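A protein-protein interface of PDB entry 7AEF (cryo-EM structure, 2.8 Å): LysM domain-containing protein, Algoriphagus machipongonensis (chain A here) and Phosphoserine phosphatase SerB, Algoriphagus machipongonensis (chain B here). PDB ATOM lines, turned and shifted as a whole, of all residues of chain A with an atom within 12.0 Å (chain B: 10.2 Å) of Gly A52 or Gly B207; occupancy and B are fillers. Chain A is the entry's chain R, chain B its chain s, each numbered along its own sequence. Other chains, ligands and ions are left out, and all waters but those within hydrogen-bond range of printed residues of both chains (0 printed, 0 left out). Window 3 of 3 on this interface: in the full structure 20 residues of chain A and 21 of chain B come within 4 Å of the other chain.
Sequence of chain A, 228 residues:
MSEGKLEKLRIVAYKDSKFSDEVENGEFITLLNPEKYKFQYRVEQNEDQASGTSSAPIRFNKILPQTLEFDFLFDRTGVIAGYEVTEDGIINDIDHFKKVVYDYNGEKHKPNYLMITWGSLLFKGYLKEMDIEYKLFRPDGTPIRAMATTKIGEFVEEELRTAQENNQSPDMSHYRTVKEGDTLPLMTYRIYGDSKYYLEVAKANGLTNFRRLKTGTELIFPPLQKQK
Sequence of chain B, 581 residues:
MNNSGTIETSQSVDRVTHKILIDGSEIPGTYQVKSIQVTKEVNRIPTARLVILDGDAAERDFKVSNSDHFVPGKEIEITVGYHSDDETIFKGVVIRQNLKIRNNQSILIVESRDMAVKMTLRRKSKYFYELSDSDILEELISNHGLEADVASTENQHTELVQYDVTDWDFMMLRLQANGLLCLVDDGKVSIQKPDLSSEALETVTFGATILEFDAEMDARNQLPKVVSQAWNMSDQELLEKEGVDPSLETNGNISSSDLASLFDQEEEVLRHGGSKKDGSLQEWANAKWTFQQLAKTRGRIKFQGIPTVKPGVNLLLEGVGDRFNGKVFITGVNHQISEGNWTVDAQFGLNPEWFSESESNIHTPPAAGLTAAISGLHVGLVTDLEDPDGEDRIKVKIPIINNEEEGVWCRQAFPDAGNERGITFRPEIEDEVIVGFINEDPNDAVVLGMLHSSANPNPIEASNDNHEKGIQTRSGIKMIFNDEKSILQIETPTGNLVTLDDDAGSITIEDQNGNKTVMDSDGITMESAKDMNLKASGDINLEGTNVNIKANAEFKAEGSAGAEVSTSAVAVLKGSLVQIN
Printed residues of chain B within 4 Å of Ala A50: Ile B210 (3.5 Å) and Leu B211 (3.97 Å). Ser A51 touches just one residue of chain B: Gly B207. Printed residues of chain B within 4 Å of Gly A52: Gly B207 (3.995 Å). Of chain B, only Ala B208 comes within 4 Å of Thr A53. Ala A56 touches none of the printed residues of chain B. No residue of chain A comes within 4 Å of Phe B206. Of the printed residues of chain A, Gly B207 touches Ser A51 and Gly A52. Ala B208 touches one residue of chain A. Of the printed residues of chain A, Leu B211 touches Ala A50 (3.97 Å). No residue of chain A comes within 4 Å of Gly B319. Asn B325 touches none of the printed residues of chain A. The nearest printed residue of chain B that does not touch Gly A52 is Ala B208 (5.8 Å). The nearest printed residue of chain A that does not touch Gly B207 is Thr A53 (4.9 Å).
Of the 21 printed residues of chain B, 4 touch a printed residue of chain A. Hydrophobic or aromatic side chains of chain B within 4 Å of the printed part of chain A: Leu B211. Hydrophobic or aromatic side chains of chain A that line the printed part of chain B: Ala A50. Among the printed residues, no Asp or Glu carboxylate lies within 4 Å of a Lys or Arg side-chain nitrogen of the other chain.
Ile B210 touches Ala A50. CB of Ala A50 touches CD2 of Leu B211, 3.97 Å away. Gly B207 touches Ser A51. O of Gly B207 touches CA of Gly A52, 3.995 Å away. CG2 of Thr A53 touches O of Ala B208, at 3.8 Å.
The side-chain amide oxygen (OE1) of Gln A49 lies within hydrogen-bond range of the side-chain hydroxyl (OG1) of Thr A53. The side-chain hydroxyl (OG1) of Thr A53 is in hydrogen-bond range of the backbone carbonyl oxygen (O) of Ala A50 (2.8 Å). The backbone carbonyl oxygen (O) of Thr B205 is in hydrogen-bond range of the backbone NH (N) of Ile B210 (3.2 Å).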
ATOM      1  N   GLU A  47      39.079  32.764  -9.660  1.00  0.00           N
ATOM      2  CA  GLU A  47      39.012  31.834 -10.784  1.00  0.00           C
ATOM      3  C   GLU A  47      37.712  31.033 -10.833  1.00  0.00           C
ATOM      4  O   GLU A  47      37.729  29.856 -11.189  1.00  0.00           O
ATOM      5  CB  GLU A  47      40.195  30.871 -10.748  1.00  0.00           C
ATOM      6  CG  GLU A  47      41.529  31.522 -10.971  1.00  0.00           C
ATOM      7  CD  GLU A  47      42.667  30.533 -10.954  1.00  0.00           C
ATOM      8  OE1 GLU A  47      42.426  29.346 -10.663  1.00  0.00           O
ATOM      9  OE2 GLU A  47      43.814  30.945 -11.227  1.00  0.00           O
ATOM     10  N   ASP A  48      36.578  31.645 -10.501  1.00  0.00           N
ATOM     11  CA  ASP A  48      35.299  30.959 -10.617  1.00  0.00           C
ATOM     12  C   ASP A  48      34.838  30.913 -12.070  1.00  0.00           C
ATOM     13  O   ASP A  48      34.952  31.899 -12.800  1.00  0.00           O
ATOM     14  CB  ASP A  48      34.243  31.656  -9.762  1.00  0.00           C
ATOM     15  CG  ASP A  48      34.492  31.499  -8.275  1.00  0.00           C
ATOM     16  OD1 ASP A  48      35.126  30.504  -7.875  1.00  0.00           O
ATOM     17  OD2 ASP A  48      34.036  32.362  -7.500  1.00  0.00           O
ATOM     18  N   GLN A  49      34.326  29.761 -12.497  1.00  0.00           N
ATOM     19  CA  GLN A  49      33.747  29.657 -13.828  1.00  0.00           C
ATOM     20  C   GLN A  49      32.537  28.740 -13.786  1.00  0.00           C
ATOM     21  O   GLN A  49      32.346  27.969 -12.847  1.00  0.00           O
ATOM     22  CB  GLN A  49      34.766  29.182 -14.878  1.00  0.00           C
ATOM     23  CG  GLN A  49      35.264  27.769 -14.744  1.00  0.00           C
ATOM     24  CD  GLN A  49      35.975  27.284 -15.992  1.00  0.00           C
ATOM     25  OE1 GLN A  49      35.441  27.345 -17.092  1.00  0.00           O
ATOM     26  NE2 GLN A  49      37.189  26.808 -15.823  1.00  0.00           N
ATOM     27  N   ALA A  50      31.708  28.854 -14.815  1.00  0.00           N
ATOM     28  CA  ALA A  50      30.499  28.057 -14.921  1.00  0.00           C
ATOM     29  C   ALA A  50      30.770  26.762 -15.674  1.00  0.00           C
ATOM     30  O   ALA A  50      31.732  26.643 -16.434  1.00  0.00           O
ATOM     31  CB  ALA A  50      29.405  28.851 -15.623  1.00  0.00           C
ATOM     32  N   SER A  51      29.903  25.782 -15.454  1.00  0.00           N
ATOM     33  CA  SER A  51      30.075  24.487 -16.089  1.00  0.00           C
ATOM     34  C   SER A  51      29.661  24.544 -17.554  1.00  0.00           C
ATOM     35  O   SER A  51      28.727  25.255 -17.925  1.00  0.00           O
ATOM     36  CB  SER A  51      29.276  23.421 -15.346  1.00  0.00           C
ATOM     37  OG  SER A  51      27.900  23.713 -15.345  1.00  0.00           O
ATOM     38  N   GLY A  52      30.372  23.793 -18.389  1.00  0.00           N
ATOM     39  CA  GLY A  52      30.142  23.783 -19.811  1.00  0.00           C
ATOM     40  C   GLY A  52      31.073  24.660 -20.609  1.00  0.00           C
ATOM     41  O   GLY A  52      30.975  24.674 -21.838  1.00  0.00           O
ATOM     42  N   THR A  53      31.971  25.382 -19.960  1.00  0.00           N
ATOM     43  CA  THR A  53      32.806  26.358 -20.634  1.00  0.00           C
ATOM     44  C   THR A  53      34.243  25.861 -20.737  1.00  0.00           C
ATOM     45  O   THR A  53      34.668  24.954 -20.022  1.00  0.00           O
ATOM     46  CB  THR A  53      32.741  27.703 -19.903  1.00  0.00           C
ATOM     47  OG1 THR A  53      33.247  27.553 -18.577  1.00  0.00           O
ATOM     48  CG2 THR A  53      31.313  28.173 -19.807  1.00  0.00           C
ATOM     49  N   SER A  54      34.997  26.468 -21.651  1.00  0.00           N
ATOM     50  CA  SER A  54      36.356  26.028 -21.928  1.00  0.00           C
ATOM     51  C   SER A  54      37.431  26.886 -21.275  1.00  0.00           C
ATOM     52  O   SER A  54      38.594  26.479 -21.272  1.00  0.00           O
ATOM     53  CB  SER A  54      36.603  25.982 -23.441  1.00  0.00           C
ATOM     54  OG  SER A  54      36.181  27.171 -24.077  1.00  0.00           O
ATOM     55  N   SER A  55      37.139  28.071 -20.797  1.00  0.00           N
ATOM     56  CA  SER A  55      38.135  28.860 -20.095  1.00  0.00           C
ATOM     57  C   SER A  55      37.465  29.884 -19.235  1.00  0.00           C
ATOM     58  O   SER A  55      36.278  30.102 -19.358  1.00  0.00           O
ATOM     59  CB  SER A  55      39.231  29.457 -20.993  1.00  0.00           C
ATOM     60  OG  SER A  55      38.757  30.048 -22.167  1.00  0.00           O
ATOM     61  N   ALA A  56      38.223  30.481 -18.328  1.00  0.00           N
ATOM     62  CA  ALA A  56      37.725  31.522 -17.444  1.00  0.00           C
ATOM     63  C   ALA A  56      38.535  32.783 -17.660  1.00  0.00           C
ATOM     64  O   ALA A  56      39.694  32.710 -18.007  1.00  0.00           O
ATOM     65  CB  ALA A  56      37.840  31.088 -15.998  1.00  0.00           C
ATOM     66  N   PRO A  57      37.916  33.960 -17.500  1.00  0.00           N
ATOM     67  CA  PRO A  57      38.766  35.145 -17.612  1.00  0.00           C
ATOM     68  C   PRO A  57      39.193  35.432 -16.194  1.00  0.00           C
ATOM     69  O   PRO A  57      38.457  36.101 -15.503  1.00  0.00           O
ATOM     70  CB  PRO A  57      37.790  36.210 -18.085  1.00  0.00           C
ATOM     71  CG  PRO A  57      36.474  35.781 -17.548  1.00  0.00           C
ATOM     72  CD  PRO A  57      36.502  34.310 -17.281  1.00  0.00           C
ATOM     73  N   SER B   4      24.414  35.179 -27.683  1.00  0.00           N
ATOM     74  CA  SER B   4      25.879  35.191 -27.685  1.00  0.00           C
ATOM     75  C   SER B   4      26.562  34.152 -26.814  1.00  0.00           C
ATOM     76  O   SER B   4      27.752  33.897 -26.975  1.00  0.00           O
ATOM     77  CB  SER B   4      26.381  36.520 -27.204  1.00  0.00           C
ATOM     78  OG  SER B   4      26.089  36.672 -25.844  1.00  0.00           O
ATOM     79  N   GLY B   5      25.847  33.573 -25.867  1.00  0.00           N
ATOM     80  CA  GLY B   5      26.430  32.601 -24.957  1.00  0.00           C
ATOM     81  C   GLY B   5      27.085  33.241 -23.743  1.00  0.00           C
ATOM     82  O   GLY B   5      27.696  32.552 -22.931  1.00  0.00           O
ATOM     83  N   THR B   6      26.996  34.555 -23.625  1.00  0.00           N
ATOM     84  CA  THR B   6      27.573  35.222 -22.482  1.00  0.00           C
ATOM     85  C   THR B   6      26.654  36.283 -21.916  1.00  0.00           C
ATOM     86  O   THR B   6      25.519  36.458 -22.356  1.00  0.00           O
ATOM     87  CB  THR B   6      28.937  35.832 -22.794  1.00  0.00           C
ATOM     88  OG1 THR B   6      29.527  36.239 -21.560  1.00  0.00           O
ATOM     89  CG2 THR B   6      28.814  37.020 -23.734  1.00  0.00           C
ATOM     90  N   THR B 203      19.063  36.667 -21.340  1.00  0.00           N
ATOM     91  CA  THR B 203      18.868  35.229 -21.344  1.00  0.00           C
ATOM     92  C   THR B 203      19.925  34.585 -20.474  1.00  0.00           C
ATOM     93  O   THR B 203      21.108  34.889 -20.602  1.00  0.00           O
ATOM     94  CB  THR B 203      18.987  34.632 -22.766  1.00  0.00           C
ATOM     95  OG1 THR B 203      18.025  35.230 -23.637  1.00  0.00           O
ATOM     96  CG2 THR B 203      18.679  33.114 -22.713  1.00  0.00           C
ATOM     97  N   VAL B 204      19.509  33.699 -19.592  1.00  0.00           N
ATOM     98  CA  VAL B 204      20.439  32.994 -18.733  1.00  0.00           C
ATOM     99  C   VAL B 204      20.340  31.496 -19.070  1.00  0.00           C
ATOM    100  O   VAL B 204      19.248  30.925 -19.054  1.00  0.00           O
ATOM    101  CB  VAL B 204      20.164  33.337 -17.252  1.00  0.00           C
ATOM    102  CG1 VAL B 204      21.102  32.626 -16.408  1.00  0.00           C
ATOM    103  CG2 VAL B 204      20.306  34.851 -17.020  1.00  0.00           C
ATOM    104  N   THR B 205      21.479  30.896 -19.443  1.00  0.00           N
ATOM    105  CA  THR B 205      21.503  29.520 -19.950  1.00  0.00           C
ATOM    106  C   THR B 205      22.315  28.518 -19.123  1.00  0.00           C
ATOM    107  O   THR B 205      23.489  28.733 -18.780  1.00  0.00           O
ATOM    108  CB  THR B 205      22.040  29.519 -21.402  1.00  0.00           C
ATOM    109  OG1 THR B 205      21.207  30.324 -22.206  1.00  0.00           O
ATOM    110  CG2 THR B 205      22.042  28.127 -21.985  1.00  0.00           C
ATOM    111  N   PHE B 206      21.719  27.368 -18.856  1.00  0.00           N
ATOM    112  CA  PHE B 206      22.410  26.341 -18.077  1.00  0.00           C
ATOM    113  C   PHE B 206      23.771  25.928 -18.587  1.00  0.00           C
ATOM    114  O   PHE B 206      24.738  25.869 -17.832  1.00  0.00           O
ATOM    115  CB  PHE B 206      21.560  25.121 -17.860  1.00  0.00           C
ATOM    116  CG  PHE B 206      22.334  24.019 -17.260  1.00  0.00           C
ATOM    117  CD1 PHE B 206      22.903  24.137 -16.019  1.00  0.00           C
ATOM    118  CD2 PHE B 206      22.478  22.839 -17.930  1.00  0.00           C
ATOM    119  CE1 PHE B 206      23.629  23.107 -15.492  1.00  0.00           C
ATOM    120  CE2 PHE B 206      23.191  21.810 -17.393  1.00  0.00           C
ATOM    121  CZ  PHE B 206      23.774  21.948 -16.180  1.00  0.00           C
ATOM    122  N   GLY B 207      23.889  25.643 -19.850  1.00  0.00           N
ATOM    123  CA  GLY B 207      25.171  25.195 -20.348  1.00  0.00           C
ATOM    124  C   GLY B 207      26.157  26.322 -20.678  1.00  0.00           C
ATOM    125  O   GLY B 207      27.196  26.052 -21.272  1.00  0.00           O
ATOM    126  N   ALA B 208      25.826  27.592 -20.383  1.00  0.00           N
ATOM    127  CA  ALA B 208      26.744  28.664 -20.749  1.00  0.00           C
ATOM    128  C   ALA B 208      26.972  29.740 -19.676  1.00  0.00           C
ATOM    129  O   ALA B 208      28.093  30.231 -19.554  1.00  0.00           O
ATOM    130  CB  ALA B 208      26.229  29.340 -22.001  1.00  0.00           C
ATOM    131  N   THR B 209      25.938  30.144 -18.923  1.00  0.00           N
ATOM    132  CA  THR B 209      26.098  31.267 -18.000  1.00  0.00           C
ATOM    133  C   THR B 209      25.712  31.015 -16.528  1.00  0.00           C
ATOM    134  O   THR B 209      26.125  31.776 -15.655  1.00  0.00           O
ATOM    135  CB  THR B 209      25.369  32.527 -18.522  1.00  0.00           C
ATOM    136  OG1 THR B 209      23.957  32.325 -18.633  1.00  0.00           O
ATOM    137  CG2 THR B 209      25.888  32.911 -19.888  1.00  0.00           C
ATOM    138  N   ILE B 210      24.964  29.954 -16.228  1.00  0.00           N
ATOM    139  CA  ILE B 210      24.531  29.684 -14.845  1.00  0.00           C
ATOM    140  C   ILE B 210      25.613  29.106 -13.932  1.00  0.00           C
ATOM    141  O   ILE B 210      26.289  28.148 -14.287  1.00  0.00           O
ATOM    142  CB  ILE B 210      23.292  28.747 -14.795  1.00  0.00           C
ATOM    143  CG1 ILE B 210      22.105  29.461 -15.410  1.00  0.00           C
ATOM    144  CG2 ILE B 210      22.991  28.270 -13.413  1.00  0.00           C
ATOM    145  CD1 ILE B 210      20.800  28.664 -15.579  1.00  0.00           C
ATOM    146  N   LEU B 211      25.760  29.690 -12.735  1.00  0.00           N
ATOM    147  CA  LEU B 211      26.710  29.217 -11.731  1.00  0.00           C
ATOM    148  C   LEU B 211      26.022  28.245 -10.767  1.00  0.00           C
ATOM    149  O   LEU B 211      26.571  27.201 -10.421  1.00  0.00           O
ATOM    150  CB  LEU B 211      27.253  30.408 -10.938  1.00  0.00           C
ATOM    151  CG  LEU B 211      28.056  31.475 -11.726  1.00  0.00           C
ATOM    152  CD1 LEU B 211      28.339  32.658 -10.819  1.00  0.00           C
ATOM    153  CD2 LEU B 211      29.354  30.897 -12.220  1.00  0.00           C
ATOM    154  N   GLU B 212      24.810  28.604 -10.337  1.00  0.00           N
ATOM    155  CA  GLU B 212      23.997  27.789  -9.412  1.00  0.00           C
ATOM    156  C   GLU B 212      22.532  27.852  -9.814  1.00  0.00           C
ATOM    157  O   GLU B 212      22.099  28.839 -10.410  1.00  0.00           O
ATOM    158  CB  GLU B 212      24.120  28.224  -7.951  1.00  0.00           C
ATOM    159  CG  GLU B 212      25.507  28.134  -7.351  1.00  0.00           C
ATOM    160  CD  GLU B 212      25.552  28.548  -5.889  1.00  0.00           C
ATOM    161  OE1 GLU B 212      24.539  28.449  -5.215  1.00  0.00           O
ATOM    162  OE2 GLU B 212      26.597  28.984  -5.447  1.00  0.00           O
ATOM    163  N   PHE B 213      21.760  26.811  -9.493  1.00  0.00           N
ATOM    164  CA  PHE B 213      20.329  26.808  -9.805  1.00  0.00           C
ATOM    165  C   PHE B 213      19.504  25.938  -8.879  1.00  0.00           C
ATOM    166  O   PHE B 213      19.875  24.802  -8.598  1.00  0.00           O
ATOM    167  CB  PHE B 213      20.120  26.343 -11.244  1.00  0.00           C
ATOM    168  CG  PHE B 213      18.705  26.358 -11.733  1.00  0.00           C
ATOM    169  CD1 PHE B 213      18.137  27.521 -12.160  1.00  0.00           C
ATOM    170  CD2 PHE B 213      17.951  25.208 -11.786  1.00  0.00           C
ATOM    171  CE1 PHE B 213      16.856  27.546 -12.620  1.00  0.00           C
ATOM    172  CE2 PHE B 213      16.669  25.236 -12.251  1.00  0.00           C
ATOM    173  CZ  PHE B 213      16.128  26.407 -12.667  1.00  0.00           C
ATOM    174  N   ILE B 301      18.308  31.698  -9.467  1.00  0.00           N
ATOM    175  CA  ILE B 301      19.310  31.585 -10.527  1.00  0.00           C
ATOM    176  C   ILE B 301      20.544  32.435 -10.183  1.00  0.00           C
ATOM    177  O   ILE B 301      20.431  33.650 -10.028  1.00  0.00           O
ATOM    178  CB  ILE B 301      18.751  32.130 -11.861  1.00  0.00           C
ATOM    179  CG1 ILE B 301      17.445  31.443 -12.244  1.00  0.00           C
ATOM    180  CG2 ILE B 301      19.762  31.811 -12.941  1.00  0.00           C
ATOM    181  CD1 ILE B 301      16.661  32.118 -13.366  1.00  0.00           C
ATOM    182  N   LEU B 317      14.800  32.080 -19.238  1.00  0.00           N
ATOM    183  CA  LEU B 317      15.510  30.916 -18.711  1.00  0.00           C
ATOM    184  C   LEU B 317      15.567  29.764 -19.706  1.00  0.00           C
ATOM    185  O   LEU B 317      14.532  29.273 -20.174  1.00  0.00           O
ATOM    186  CB  LEU B 317      14.835  30.483 -17.398  1.00  0.00           C
ATOM    187  CG  LEU B 317      15.326  29.184 -16.690  1.00  0.00           C
ATOM    188  CD1 LEU B 317      16.791  29.307 -16.224  1.00  0.00           C
ATOM    189  CD2 LEU B 317      14.399  28.932 -15.490  1.00  0.00           C
ATOM    190  N   GLU B 318      16.784  29.314 -20.021  1.00  0.00           N
ATOM    191  CA  GLU B 318      16.974  28.223 -20.971  1.00  0.00           C
ATOM    192  C   GLU B 318      17.918  27.113 -20.512  1.00  0.00           C
ATOM    193  O   GLU B 318      18.859  27.342 -19.748  1.00  0.00           O
ATOM    194  CB  GLU B 318      17.490  28.763 -22.302  1.00  0.00           C
ATOM    195  CG  GLU B 318      16.521  29.662 -23.038  1.00  0.00           C
ATOM    196  CD  GLU B 318      17.034  30.105 -24.379  1.00  0.00           C
ATOM    197  OE1 GLU B 318      18.205  29.968 -24.608  1.00  0.00           O
ATOM    198  OE2 GLU B 318      16.250  30.532 -25.198  1.00  0.00           O
ATOM    199  N   GLY B 319      17.683  25.914 -21.044  1.00  0.00           N
ATOM    200  CA  GLY B 319      18.542  24.756 -20.821  1.00  0.00           C
ATOM    201  C   GLY B 319      18.317  23.965 -19.534  1.00  0.00           C
ATOM    202  O   GLY B 319      19.189  23.189 -19.155  1.00  0.00           O
ATOM    203  N   VAL B 320      17.173  24.123 -18.865  1.00  0.00           N
ATOM    204  CA  VAL B 320      16.937  23.410 -17.605  1.00  0.00           C
ATOM    205  C   VAL B 320      15.763  22.431 -17.663  1.00  0.00           C
ATOM    206  O   VAL B 320      15.216  22.044 -16.636  1.00  0.00           O
ATOM    207  CB  VAL B 320      16.719  24.387 -16.428  1.00  0.00           C
ATOM    208  CG1 VAL B 320      17.981  25.199 -16.152  1.00  0.00           C
ATOM    209  CG2 VAL B 320      15.586  25.320 -16.739  1.00  0.00           C
ATOM    210  N   GLY B 321      15.372  22.048 -18.863  1.00  0.00           N
ATOM    211  CA  GLY B 321      14.278  21.109 -19.065  1.00  0.00           C
ATOM    212  C   GLY B 321      12.939  21.780 -19.344  1.00  0.00           C
ATOM    213  O   GLY B 321      12.625  22.848 -18.811  1.00  0.00           O
ATOM    214  N   ASN B 325      11.698  25.614 -18.400  1.00  0.00           N
ATOM    215  CA  ASN B 325      12.119  26.616 -19.390  1.00  0.00           C
ATOM    216  C   ASN B 325      11.030  27.636 -19.732  1.00  0.00           C
ATOM    217  O   ASN B 325       9.832  27.314 -19.736  1.00  0.00           O
ATOM    218  CB  ASN B 325      12.570  25.964 -20.681  1.00  0.00           C
ATOM    219  CG  ASN B 325      13.874  25.232 -20.624  1.00  0.00           C
ATOM    220  OD1 ASN B 325      14.804  25.526 -19.859  1.00  0.00           O
ATOM    221  ND2 ASN B 325      13.957  24.260 -21.475  1.00  0.00           N
